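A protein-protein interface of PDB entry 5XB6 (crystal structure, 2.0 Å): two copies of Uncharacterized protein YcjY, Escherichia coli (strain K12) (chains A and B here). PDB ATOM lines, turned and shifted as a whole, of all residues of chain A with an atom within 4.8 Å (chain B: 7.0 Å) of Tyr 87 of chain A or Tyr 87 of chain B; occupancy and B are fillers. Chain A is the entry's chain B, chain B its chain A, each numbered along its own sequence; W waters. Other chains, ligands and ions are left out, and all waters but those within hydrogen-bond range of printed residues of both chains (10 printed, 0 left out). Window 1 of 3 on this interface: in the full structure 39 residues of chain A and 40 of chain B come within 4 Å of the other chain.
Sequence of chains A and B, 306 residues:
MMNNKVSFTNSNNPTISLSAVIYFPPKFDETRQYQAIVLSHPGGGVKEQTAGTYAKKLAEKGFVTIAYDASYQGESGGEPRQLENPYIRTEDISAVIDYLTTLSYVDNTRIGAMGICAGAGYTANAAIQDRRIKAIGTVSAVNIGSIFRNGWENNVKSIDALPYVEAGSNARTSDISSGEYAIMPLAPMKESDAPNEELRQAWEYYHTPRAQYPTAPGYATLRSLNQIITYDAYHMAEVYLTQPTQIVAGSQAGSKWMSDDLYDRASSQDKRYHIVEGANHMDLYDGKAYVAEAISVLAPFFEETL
The side-chain amide nitrogen (ND2) of Asn 85 of chain B sits at hydrogen-bond distance from the side-chain carboxylate (OE1) of Glu 91 of chain A.
The side-chain carboxylate (OE2) of Glu 91 of chain B sits close to the side-chain amide oxygen (OE1) of Gln 227 of chain A.
The side-chain amide nitrogen (ND2) of Asn 12 of chain B sits at hydrogen-bond distance from the backbone carbonyl oxygen (O) of Glu 91 of chain B (2.9 Å).
The backbone NH of Ile 88 of chain B is in hydrogen-bond range of the side-chain amide oxygen of Asn 85 of chain B, 3.4 Å away.
The backbone carbonyl oxygen (O) of Gln 227 of chain B lies within hydrogen-bond range of the side-chain hydroxyl (OG1) of Thr 230 of chain B.
The backbone NH (N) of Tyr 87 of chain A lies within hydrogen-bond range of the side-chain amide oxygen (OD1) of Asn 85 of chain A (3.0 Å).
OD1 of Asn 85 of chain A lies within hydrogen-bond range of N of Ile 88 of chain A (3.4 Å).
The side-chain amide nitrogen (NE2) of Gln 227 of chain A lies close to the side-chain amide nitrogen (ND2) of Asn 85 of chain A (3.3 Å).
ND2 of Asn 85 of chain A touches OE1 of Glu 91 of chain B, 3.6 Å away.
Tyr 87 of chain A touches Tyr 87 of chain B.
Gln 227 of chain B touches Glu 91 of chain A (NE2 to CD, 3.3 Å).
Gln 129 of chain B touches Gln 227 of chain A.
OG1 of Thr 230 of chain A touches CB of Gln 129 of chain B, at 3.7 Å.
Thr 230 of chain A touches His 235 of chain B.
Of the printed residues of chain B, Asn 85 of chain A touches Glu 91 (3.6 Å).
Of chain B, only Tyr 87 (3.3 Å) comes within 4 Å of Tyr 87 of chain A.
Of the printed residues of chain A, Asn 85 of chain B touches Glu 91 (3.4 Å).
Of the printed residues of chain A, Tyr 87 of chain B touches Tyr 87 (3.3 Å).
Of the printed residues of chain A, His 235 of chain B touches Thr 230 (3.97 Å).
Hydrophobic or aromatic side chains of chain B within 4 Å of the printed part of chain A: Tyr 87 and His 235.
Of the 10 printed residues of chain A, 5 touch a printed residue of chain B.
Printed residues of chain A that touch a printed residue of chain B: Asn 85, Tyr 87, Glu 91, Gln 227 and Thr 230.
Among the printed residues, 8 pairs touch across the chains.
Among the printed residues, no Asp or Glu carboxylate lies within 4 Å of a Lys or Arg side-chain nitrogen of the other chain.
Asn 85 of chain A touches Glu 91 of chain B, and with the chains exchanged Glu 91 of chain A touches Asn 85 of chain B.
Tyr 87 of chain A touches its own counterpart, Tyr 87 of chain B.
Glu 91 of chain A touches Gln 227 of chain B, and with the chains exchanged Gln 227 of chain A touches Glu 91 of chain B.
Water W8 lies within hydrogen-bond range of OG1 of Thr 230 of chain A (2.6 Å), OH of Tyr 87 of chain A (2.7 Å), O of Gln 227 of chain A (3.0 Å) and OE1 of Gln 129 of chain B (3.0 Å).
Water W9 bridges OE1 of Glu 91 of chain A and ND2 of Asn 85 of chain B.
Water W2 lies within hydrogen-bond range of the backbone carbonyl oxygen (O) of Tyr 87 of chain B (2.9 Å), the side-chain amide nitrogen (NE2) of Gln 129 of chain B (3.0 Å) and the side-chain amide nitrogen (NE2) of Gln 227 of chain A (3.1 Å).
Water W6 lies within hydrogen-bond range of O of Tyr 87 of chain A (2.9 Å) and NE2 of Gln 227 of chain B (3.1 Å).
Water W10 lies within hydrogen-bond range of the side-chain amide nitrogen of Asn 85 of chain B, the side-chain carboxylate of Glu 91 of chain A, the backbone carbonyl oxygen of Tyr 87 of chain A and the side-chain amide nitrogen of Gln 227 of chain B.
Water W1 lies within hydrogen-bond range of ND2 of Asn 85 of chain A (3.0 Å), O of Tyr 87 of chain B (3.2 Å), OE1 of Glu 91 of chain B (3.3 Å) and NE2 of Gln 227 of chain A (3.5 Å).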
ATOM      1  N   ASN A  85     -30.186 -12.739  14.976  1.00  0.00           N
ATOM      2  CA  ASN A  85     -29.457 -11.572  14.500  1.00  0.00           C
ATOM      3  C   ASN A  85     -30.199 -11.051  13.282  1.00  0.00           C
ATOM      4  O   ASN A  85     -30.238 -11.722  12.258  1.00  0.00           O
ATOM      5  CB  ASN A  85     -28.027 -11.976  14.128  1.00  0.00           C
ATOM      6  CG  ASN A  85     -27.180 -10.807  13.686  1.00  0.00           C
ATOM      7  OD1 ASN A  85     -27.684  -9.852  13.100  1.00  0.00           O
ATOM      8  ND2 ASN A  85     -25.870 -10.882  13.950  1.00  0.00           N
ATOM      9  N   PRO A  86     -30.782  -9.840  13.378  1.00  0.00           N
ATOM     10  CA  PRO A  86     -31.684  -9.356  12.325  1.00  0.00           C
ATOM     11  C   PRO A  86     -30.950  -9.055  11.026  1.00  0.00           C
ATOM     12  O   PRO A  86     -31.542  -9.133   9.935  1.00  0.00           O
ATOM     13  CB  PRO A  86     -32.276  -8.076  12.930  1.00  0.00           C
ATOM     14  CG  PRO A  86     -31.243  -7.604  13.915  1.00  0.00           C
ATOM     15  CD  PRO A  86     -30.644  -8.871  14.484  1.00  0.00           C
ATOM     16  N   TYR A  87     -29.659  -8.748  11.137  1.00  0.00           N
ATOM     17  CA  TYR A  87     -28.815  -8.534   9.955  1.00  0.00           C
ATOM     18  C   TYR A  87     -28.535  -9.835   9.201  1.00  0.00           C
ATOM     19  O   TYR A  87     -28.465  -9.874   7.963  1.00  0.00           O
ATOM     20  CB  TYR A  87     -27.518  -7.829  10.374  1.00  0.00           C
ATOM     21  CG  TYR A  87     -27.832  -6.580  11.148  1.00  0.00           C
ATOM     22  CD1 TYR A  87     -28.505  -5.532  10.538  1.00  0.00           C
ATOM     23  CD2 TYR A  87     -27.496  -6.461  12.496  1.00  0.00           C
ATOM     24  CE1 TYR A  87     -28.835  -4.388  11.237  1.00  0.00           C
ATOM     25  CE2 TYR A  87     -27.814  -5.309  13.207  1.00  0.00           C
ATOM     26  CZ  TYR A  87     -28.483  -4.279  12.564  1.00  0.00           C
ATOM     27  OH  TYR A  87     -28.808  -3.124  13.241  1.00  0.00           O
ATOM     28  N   ILE A  88     -28.410 -10.908   9.960  1.00  0.00           N
ATOM     29  CA  ILE A  88     -28.219 -12.219   9.383  1.00  0.00           C
ATOM     30  C   ILE A  88     -29.540 -12.714   8.812  1.00  0.00           C
ATOM     31  O   ILE A  88     -29.575 -13.231   7.703  1.00  0.00           O
ATOM     32  CB  ILE A  88     -27.676 -13.191  10.428  1.00  0.00           C
ATOM     33  CG1 ILE A  88     -26.308 -12.701  10.927  1.00  0.00           C
ATOM     34  CG2 ILE A  88     -27.568 -14.597   9.853  1.00  0.00           C
ATOM     35  CD1 ILE A  88     -25.684 -13.646  11.967  1.00  0.00           C
ATOM     36  N   ARG A  89     -30.638 -12.552   9.554  1.00  0.00           N
ATOM     37  CA  ARG A  89     -31.945 -12.941   9.007  1.00  0.00           C
ATOM     38  C   ARG A  89     -32.196 -12.216   7.691  1.00  0.00           C
ATOM     39  O   ARG A  89     -32.743 -12.794   6.740  1.00  0.00           O
ATOM     40  CB  ARG A  89     -33.073 -12.653  10.001  1.00  0.00           C
ATOM     41  CG  ARG A  89     -33.033 -13.539  11.245  1.00  0.00           C
ATOM     42  CD  ARG A  89     -33.747 -14.867  11.016  1.00  0.00           C
ATOM     43  NE  ARG A  89     -35.176 -14.819  11.357  1.00  0.00           N
ATOM     44  CZ  ARG A  89     -36.169 -15.014  10.489  1.00  0.00           C
ATOM     45  NH1 ARG A  89     -35.907 -15.264   9.212  1.00  0.00           N
ATOM     46  NH2 ARG A  89     -37.439 -14.960  10.891  1.00  0.00           N
ATOM     47  N   THR A  90     -31.798 -10.946   7.622  1.00  0.00           N
ATOM     48  CA  THR A  90     -31.968 -10.208   6.369  1.00  0.00           C
ATOM     49  C   THR A  90     -31.056 -10.766   5.258  1.00  0.00           C
ATOM     50  O   THR A  90     -31.518 -11.040   4.143  1.00  0.00           O
ATOM     51  CB  THR A  90     -31.710  -8.690   6.537  1.00  0.00           C
ATOM     52  OG1 THR A  90     -32.680  -8.125   7.440  1.00  0.00           O
ATOM     53  CG2 THR A  90     -31.820  -7.981   5.175  1.00  0.00           C
ATOM     54  N   GLU A  91     -29.771 -10.947   5.562  1.00  0.00           N
ATOM     55  CA  GLU A  91     -28.800 -11.406   4.543  1.00  0.00           C
ATOM     56  C   GLU A  91     -29.073 -12.830   4.007  1.00  0.00           C
ATOM     57  O   GLU A  91     -28.745 -13.163   2.843  1.00  0.00           O
ATOM     58  CB  GLU A  91     -27.347 -11.275   5.059  1.00  0.00           C
ATOM     59  CG  GLU A  91     -26.389 -10.807   3.945  1.00  0.00           C
ATOM     60  CD  GLU A  91     -24.892 -10.942   4.271  1.00  0.00           C
ATOM     61  OE1 GLU A  91     -24.511 -11.320   5.406  1.00  0.00           O
ATOM     62  OE2 GLU A  91     -24.086 -10.655   3.355  1.00  0.00           O
ATOM     63  N   GLN A 227     -29.233  -6.203  19.614  1.00  0.00           N
ATOM     64  CA  GLN A 227     -29.227  -5.846  18.196  1.00  0.00           C
ATOM     65  C   GLN A 227     -30.660  -5.578  17.742  1.00  0.00           C
ATOM     66  O   GLN A 227     -30.915  -4.692  16.927  1.00  0.00           O
ATOM     67  CB  GLN A 227     -28.614  -6.959  17.348  1.00  0.00           C
ATOM     68  CG  GLN A 227     -27.093  -7.116  17.487  1.00  0.00           C
ATOM     69  CD  GLN A 227     -26.585  -8.336  16.740  1.00  0.00           C
ATOM     70  OE1 GLN A 227     -26.973  -9.474  17.041  1.00  0.00           O
ATOM     71  NE2 GLN A 227     -25.727  -8.108  15.752  1.00  0.00           N
ATOM     72  N   THR A 230     -32.075  -2.070  18.581  1.00  0.00           N
ATOM     73  CA  THR A 230     -31.444  -1.002  17.812  1.00  0.00           C
ATOM     74  C   THR A 230     -31.560  -1.220  16.297  1.00  0.00           C
ATOM     75  O   THR A 230     -30.807  -0.636  15.520  1.00  0.00           O
ATOM     76  CB  THR A 230     -29.969  -0.837  18.217  1.00  0.00           C
ATOM     77  OG1 THR A 230     -29.305  -2.106  18.142  1.00  0.00           O
ATOM     78  CG2 THR A 230     -29.880  -0.321  19.654  1.00  0.00           C
ATOM     79  N   TYR A 231     -32.523  -2.049  15.893  1.00  0.00           N
ATOM     80  CA  TYR A 231     -32.710  -2.442  14.492  1.00  0.00           C
ATOM     81  C   TYR A 231     -33.969  -1.800  13.924  1.00  0.00           C
ATOM     82  O   TYR A 231     -34.955  -1.613  14.644  1.00  0.00           O
ATOM     83  CB  TYR A 231     -32.851  -3.975  14.419  1.00  0.00           C
ATOM     84  CG  TYR A 231     -33.197  -4.526  13.056  1.00  0.00           C
ATOM     85  CD1 TYR A 231     -32.258  -4.530  12.023  1.00  0.00           C
ATOM     86  CD2 TYR A 231     -34.451  -5.073  12.801  1.00  0.00           C
ATOM     87  CE1 TYR A 231     -32.569  -5.037  10.772  1.00  0.00           C
ATOM     88  CE2 TYR A 231     -34.773  -5.592  11.552  1.00  0.00           C
ATOM     89  CZ  TYR A 231     -33.831  -5.577  10.547  1.00  0.00           C
ATOM     90  OH  TYR A 231     -34.156  -6.097   9.305  1.00  0.00           O
ATOM     91  N   ASN B  12     -19.731 -14.564  18.853  1.00  0.00           N
ATOM     92  CA  ASN B  12     -20.826 -14.370  17.884  1.00  0.00           C
ATOM     93  C   ASN B  12     -20.876 -15.466  16.840  1.00  0.00           C
ATOM     94  O   ASN B  12     -21.936 -15.789  16.307  1.00  0.00           O
ATOM     95  CB  ASN B  12     -20.686 -13.032  17.156  1.00  0.00           C
ATOM     96  CG  ASN B  12     -20.575 -11.875  18.108  1.00  0.00           C
ATOM     97  OD1 ASN B  12     -21.116 -11.927  19.215  1.00  0.00           O
ATOM     98  ND2 ASN B  12     -19.853 -10.832  17.705  1.00  0.00           N
ATOM     99  N   GLU B  84     -16.283  -7.161   4.414  1.00  0.00           N
ATOM    100  CA  GLU B  84     -16.529  -5.920   5.143  1.00  0.00           C
ATOM    101  C   GLU B  84     -18.020  -5.792   5.424  1.00  0.00           C
ATOM    102  O   GLU B  84     -18.696  -4.867   4.955  1.00  0.00           O
ATOM    103  CB  GLU B  84     -15.978  -4.695   4.403  1.00  0.00           C
ATOM    104  CG  GLU B  84     -15.935  -3.417   5.262  1.00  0.00           C
ATOM    105  CD  GLU B  84     -14.889  -3.472   6.376  1.00  0.00           C
ATOM    106  OE1 GLU B  84     -13.898  -4.230   6.250  1.00  0.00           O
ATOM    107  OE2 GLU B  84     -15.063  -2.748   7.382  1.00  0.00           O
ATOM    108  N   ASN B  85     -18.523  -6.754   6.184  1.00  0.00           N
ATOM    109  CA  ASN B  85     -19.875  -6.708   6.710  1.00  0.00           C
ATOM    110  C   ASN B  85     -19.879  -5.775   7.917  1.00  0.00           C
ATOM    111  O   ASN B  85     -19.364  -6.122   8.984  1.00  0.00           O
ATOM    112  CB  ASN B  85     -20.332  -8.124   7.110  1.00  0.00           C
ATOM    113  CG  ASN B  85     -21.813  -8.181   7.475  1.00  0.00           C
ATOM    114  OD1 ASN B  85     -22.358  -7.207   7.992  1.00  0.00           O
ATOM    115  ND2 ASN B  85     -22.468  -9.326   7.220  1.00  0.00           N
ATOM    116  N   PRO B  86     -20.481  -4.592   7.762  1.00  0.00           N
ATOM    117  CA  PRO B  86     -20.414  -3.572   8.820  1.00  0.00           C
ATOM    118  C   PRO B  86     -21.086  -4.018  10.122  1.00  0.00           C
ATOM    119  O   PRO B  86     -20.636  -3.645  11.223  1.00  0.00           O
ATOM    120  CB  PRO B  86     -21.167  -2.381   8.203  1.00  0.00           C
ATOM    121  CG  PRO B  86     -22.060  -2.994   7.158  1.00  0.00           C
ATOM    122  CD  PRO B  86     -21.292  -4.157   6.609  1.00  0.00           C
ATOM    123  N   TYR B  87     -22.134  -4.832  10.006  1.00  0.00           N
ATOM    124  CA  TYR B  87     -22.799  -5.374  11.190  1.00  0.00           C
ATOM    125  C   TYR B  87     -21.902  -6.341  11.940  1.00  0.00           C
ATOM    126  O   TYR B  87     -21.923  -6.388  13.181  1.00  0.00           O
ATOM    127  CB  TYR B  87     -24.150  -6.005  10.807  1.00  0.00           C
ATOM    128  CG  TYR B  87     -24.969  -5.028  10.001  1.00  0.00           C
ATOM    129  CD1 TYR B  87     -25.450  -3.860  10.582  1.00  0.00           C
ATOM    130  CD2 TYR B  87     -25.229  -5.246   8.657  1.00  0.00           C
ATOM    131  CE1 TYR B  87     -26.184  -2.949   9.844  1.00  0.00           C
ATOM    132  CE2 TYR B  87     -25.957  -4.334   7.908  1.00  0.00           C
ATOM    133  CZ  TYR B  87     -26.431  -3.190   8.512  1.00  0.00           C
ATOM    134  OH  TYR B  87     -27.154  -2.269   7.773  1.00  0.00           O
ATOM    135  N   ILE B  88     -21.100  -7.104  11.190  1.00  0.00           N
ATOM    136  CA  ILE B  88     -20.142  -8.026  11.794  1.00  0.00           C
ATOM    137  C   ILE B  88     -18.969  -7.261  12.408  1.00  0.00           C
ATOM    138  O   ILE B  88     -18.543  -7.567  13.515  1.00  0.00           O
ATOM    139  CB  ILE B  88     -19.618  -9.074  10.785  1.00  0.00           C
ATOM    140  CG1 ILE B  88     -20.768  -9.971  10.331  1.00  0.00           C
ATOM    141  CG2 ILE B  88     -18.490  -9.923  11.406  1.00  0.00           C
ATOM    142  CD1 ILE B  88     -20.342 -11.084   9.400  1.00  0.00           C
ATOM    143  N   ARG B  89     -18.445  -6.277  11.685  1.00  0.00           N
ATOM    144  CA  ARG B  89     -17.366  -5.438  12.214  1.00  0.00           C
ATOM    145  C   ARG B  89     -17.806  -4.793  13.521  1.00  0.00           C
ATOM    146  O   ARG B  89     -17.026  -4.671  14.469  1.00  0.00           O
ATOM    147  CB  ARG B  89     -16.989  -4.347  11.206  1.00  0.00           C
ATOM    148  CG  ARG B  89     -16.295  -4.864   9.970  1.00  0.00           C
ATOM    149  CD  ARG B  89     -14.799  -5.083  10.209  1.00  0.00           C
ATOM    150  NE  ARG B  89     -13.984  -3.921   9.855  1.00  0.00           N
ATOM    151  CZ  ARG B  89     -13.265  -3.195  10.718  1.00  0.00           C
ATOM    152  NH1 ARG B  89     -13.235  -3.511  12.003  1.00  0.00           N
ATOM    153  NH2 ARG B  89     -12.551  -2.158  10.284  1.00  0.00           N
ATOM    154  N   THR B  90     -19.068  -4.387  13.571  1.00  0.00           N
ATOM    155  CA  THR B  90     -19.613  -3.824  14.797  1.00  0.00           C
ATOM    156  C   THR B  90     -19.708  -4.876  15.897  1.00  0.00           C
ATOM    157  O   THR B  90     -19.230  -4.643  17.016  1.00  0.00           O
ATOM    158  CB  THR B  90     -20.993  -3.191  14.587  1.00  0.00           C
ATOM    159  OG1 THR B  90     -20.865  -2.044  13.745  1.00  0.00           O
ATOM    160  CG2 THR B  90     -21.584  -2.747  15.925  1.00  0.00           C
ATOM    161  N   GLU B  91     -20.308  -6.033  15.599  1.00  0.00           N
ATOM    162  CA  GLU B  91     -20.477  -7.063  16.641  1.00  0.00           C
ATOM    163  C   GLU B  91     -19.159  -7.645  17.182  1.00  0.00           C
ATOM    164  O   GLU B  91     -19.078  -8.155  18.328  1.00  0.00           O
ATOM    165  CB  GLU B  91     -21.428  -8.179  16.187  1.00  0.00           C
ATOM    166  CG  GLU B  91     -22.302  -8.684  17.353  1.00  0.00           C
ATOM    167  CD  GLU B  91     -23.078  -9.955  17.046  1.00  0.00           C
ATOM    168  OE1 GLU B  91     -22.895 -10.543  15.957  1.00  0.00           O
ATOM    169  OE2 GLU B  91     -23.869 -10.373  17.915  1.00  0.00           O
ATOM    170  N   ASP B  92     -18.119  -7.553  16.357  1.00  0.00           N
ATOM    171  CA  ASP B  92     -16.792  -8.040  16.725  1.00  0.00           C
ATOM    172  C   ASP B  92     -16.409  -7.417  18.047  1.00  0.00           C
ATOM    173  O   ASP B  92     -15.855  -8.080  18.922  1.00  0.00           O
ATOM    174  CB  ASP B  92     -15.747  -7.653  15.660  1.00  0.00           C
ATOM    175  CG  ASP B  92     -15.686  -8.638  14.489  1.00  0.00           C
ATOM    176  OD1 ASP B  92     -16.243  -9.750  14.607  1.00  0.00           O
ATOM    177  OD2 ASP B  92     -15.057  -8.300  13.452  1.00  0.00           O
ATOM    178  N   TYR B 122     -17.619   2.075  13.667  1.00  0.00           N
ATOM    179  CA  TYR B 122     -18.037   0.819  14.252  1.00  0.00           C
ATOM    180  C   TYR B 122     -18.092   0.947  15.770  1.00  0.00           C
ATOM    181  O   TYR B 122     -19.043   0.480  16.401  1.00  0.00           O
ATOM    182  CB  TYR B 122     -17.079  -0.286  13.825  1.00  0.00           C
ATOM    183  CG  TYR B 122     -17.118  -0.562  12.335  1.00  0.00           C
ATOM    184  CD1 TYR B 122     -18.331  -0.586  11.643  1.00  0.00           C
ATOM    185  CD2 TYR B 122     -15.955  -0.796  11.626  1.00  0.00           C
ATOM    186  CE1 TYR B 122     -18.380  -0.843  10.280  1.00  0.00           C
ATOM    187  CE2 TYR B 122     -15.986  -1.058  10.258  1.00  0.00           C
ATOM    188  CZ  TYR B 122     -17.201  -1.077   9.596  1.00  0.00           C
ATOM    189  OH  TYR B 122     -17.234  -1.350   8.248  1.00  0.00           O
ATOM    190  N   ASN B 125     -21.099   2.522  16.724  1.00  0.00           N
ATOM    191  CA  ASN B 125     -22.250   1.653  16.546  1.00  0.00           C
ATOM    192  C   ASN B 125     -22.237   0.643  17.691  1.00  0.00           C
ATOM    193  O   ASN B 125     -23.273   0.346  18.294  1.00  0.00           O
ATOM    194  CB  ASN B 125     -22.155   0.955  15.183  1.00  0.00           C
ATOM    195  CG  ASN B 125     -23.383   0.139  14.849  1.00  0.00           C
ATOM    196  OD1 ASN B 125     -24.155  -0.226  15.739  1.00  0.00           O
ATOM    197  ND2 ASN B 125     -23.574  -0.158  13.562  1.00  0.00           N
ATOM    198  N   GLN B 129     -25.274  -0.336  20.775  1.00  0.00           N
ATOM    199  CA  GLN B 129     -25.976  -1.591  21.043  1.00  0.00           C
ATOM    200  C   GLN B 129     -25.394  -2.367  22.212  1.00  0.00           C
ATOM    201  O   GLN B 129     -26.065  -3.226  22.777  1.00  0.00           O
ATOM    202  CB  GLN B 129     -26.048  -2.465  19.783  1.00  0.00           C
ATOM    203  CG  GLN B 129     -24.693  -2.923  19.248  1.00  0.00           C
ATOM    204  CD  GLN B 129     -24.829  -3.759  17.984  1.00  0.00           C
ATOM    205  OE1 GLN B 129     -25.793  -3.610  17.235  1.00  0.00           O
ATOM    206  NE2 GLN B 129     -23.867  -4.651  17.750  1.00  0.00           N
ATOM    207  N   GLN B 227     -24.465  -3.780   1.438  1.00  0.00           N
ATOM    208  CA  GLN B 227     -24.752  -3.563   2.856  1.00  0.00           C
ATOM    209  C   GLN B 227     -24.086  -2.283   3.340  1.00  0.00           C
ATOM    210  O   GLN B 227     -24.595  -1.620   4.246  1.00  0.00           O
ATOM    211  CB  GLN B 227     -24.234  -4.709   3.733  1.00  0.00           C
ATOM    212  CG  GLN B 227     -24.986  -6.028   3.628  1.00  0.00           C
ATOM    213  CD  GLN B 227     -24.280  -7.144   4.396  1.00  0.00           C
ATOM    214  OE1 GLN B 227     -23.083  -7.392   4.203  1.00  0.00           O
ATOM    215  NE2 GLN B 227     -25.013  -7.811   5.278  1.00  0.00           N
ATOM    216  N   ILE B 228     -22.936  -1.944   2.761  1.00  0.00           N
ATOM    217  CA  ILE B 228     -22.218  -0.771   3.257  1.00  0.00           C
ATOM    218  C   ILE B 228     -22.975   0.503   2.901  1.00  0.00           C
ATOM    219  O   ILE B 228     -23.125   1.406   3.727  1.00  0.00           O
ATOM    220  CB  ILE B 228     -20.787  -0.729   2.714  1.00  0.00           C
ATOM    221  CG1 ILE B 228     -19.982  -1.854   3.360  1.00  0.00           C
ATOM    222  CG2 ILE B 228     -20.141   0.636   2.969  1.00  0.00           C
ATOM    223  CD1 ILE B 228     -18.634  -2.098   2.708  1.00  0.00           C
ATOM    224  N   THR B 230     -26.062   0.914   2.441  1.00  0.00           N
ATOM    225  CA  THR B 230     -27.299   1.029   3.196  1.00  0.00           C
ATOM    226  C   THR B 230     -27.013   0.952   4.703  1.00  0.00           C
ATOM    227  O   THR B 230     -27.911   0.678   5.502  1.00  0.00           O
ATOM    228  CB  THR B 230     -28.330  -0.034   2.762  1.00  0.00           C
ATOM    229  OG1 THR B 230     -27.758  -1.337   2.904  1.00  0.00           O
ATOM    230  CG2 THR B 230     -28.744   0.163   1.291  1.00  0.00           C
ATOM    231  N   TYR B 231     -25.760   1.205   5.079  1.00  0.00           N
ATOM    232  CA  TYR B 231     -25.338   1.187   6.483  1.00  0.00           C
ATOM    233  C   TYR B 231     -25.170   2.606   7.049  1.00  0.00           C
ATOM    234  O   TYR B 231     -24.722   3.524   6.346  1.00  0.00           O
ATOM    235  CB  TYR B 231     -24.020   0.405   6.623  1.00  0.00           C
ATOM    236  CG  TYR B 231     -23.419   0.417   8.024  1.00  0.00           C
ATOM    237  CD1 TYR B 231     -24.011  -0.282   9.062  1.00  0.00           C
ATOM    238  CD2 TYR B 231     -22.241   1.112   8.293  1.00  0.00           C
ATOM    239  CE1 TYR B 231     -23.463  -0.281  10.339  1.00  0.00           C
ATOM    240  CE2 TYR B 231     -21.681   1.120   9.563  1.00  0.00           C
ATOM    241  CZ  TYR B 231     -22.296   0.421  10.580  1.00  0.00           C
ATOM    242  OH  TYR B 231     -21.731   0.438  11.842  1.00  0.00           O
ATOM    243  N   ASP B 232     -25.537   2.785   8.317  1.00  0.00           N
ATOM    244  CA  ASP B 232     -25.277   4.035   9.031  1.00  0.00           C
ATOM    245  C   ASP B 232     -24.675   3.723  10.393  1.00  0.00           C
ATOM    246  O   ASP B 232     -25.364   3.223  11.276  1.00  0.00           O
ATOM    247  CB  ASP B 232     -26.571   4.820   9.191  1.00  0.00           C
ATOM    248  CG  ASP B 232     -26.396   6.110   9.977  1.00  0.00           C
ATOM    249  OD1 ASP B 232     -25.248   6.498  10.297  1.00  0.00           O
ATOM    250  OD2 ASP B 232     -27.434   6.754  10.253  1.00  0.00           O
ATOM    251  N   HIS B 235     -26.553   4.988  13.464  1.00  0.00           N
ATOM    252  CA  HIS B 235     -27.989   4.703  13.471  1.00  0.00           C
ATOM    253  C   HIS B 235     -28.558   4.692  14.895  1.00  0.00           C
ATOM    254  O   HIS B 235     -28.118   3.910  15.730  1.00  0.00           O
ATOM    255  CB  HIS B 235     -28.245   3.360  12.784  1.00  0.00           C
ATOM    256  CG  HIS B 235     -29.691   3.069  12.535  1.00  0.00           C
ATOM    257  ND1 HIS B 235     -30.183   1.786  12.431  1.00  0.00           N
ATOM    258  CD2 HIS B 235     -30.750   3.895  12.366  1.00  0.00           C
ATOM    259  CE1 HIS B 235     -31.485   1.832  12.212  1.00  0.00           C
ATOM    260  NE2 HIS B 235     -31.855   3.100  12.168  1.00  0.00           N
HETATM  261  O   HOH W   1     -23.646  -9.055  13.110  1.00  0.00           O
HETATM  262  O   HOH W   2     -24.041  -5.610  14.958  1.00  0.00           O
HETATM  263  O   HOH W   3     -28.404   0.687  14.972  1.00  0.00           O
HETATM  264  O   HOH W   4     -26.702  -1.274  14.829  1.00  0.00           O
HETATM  265  O   HOH W   5     -24.197 -12.693  15.541  1.00  0.00           O
HETATM  266  O   HOH W   6     -27.998  -7.671   6.148  1.00  0.00           O
HETATM  267  O   HOH W   7     -28.577  -0.384  12.158  1.00  0.00           O
HETATM  268  O   HOH W   8     -28.507  -3.290  15.916  1.00  0.00           O
HETATM  269  O   HOH W   9     -21.879 -11.619   5.759  1.00  0.00           O
HETATM  270  O   HOH W  10     -25.321  -9.761   7.915  1.00  0.00           O
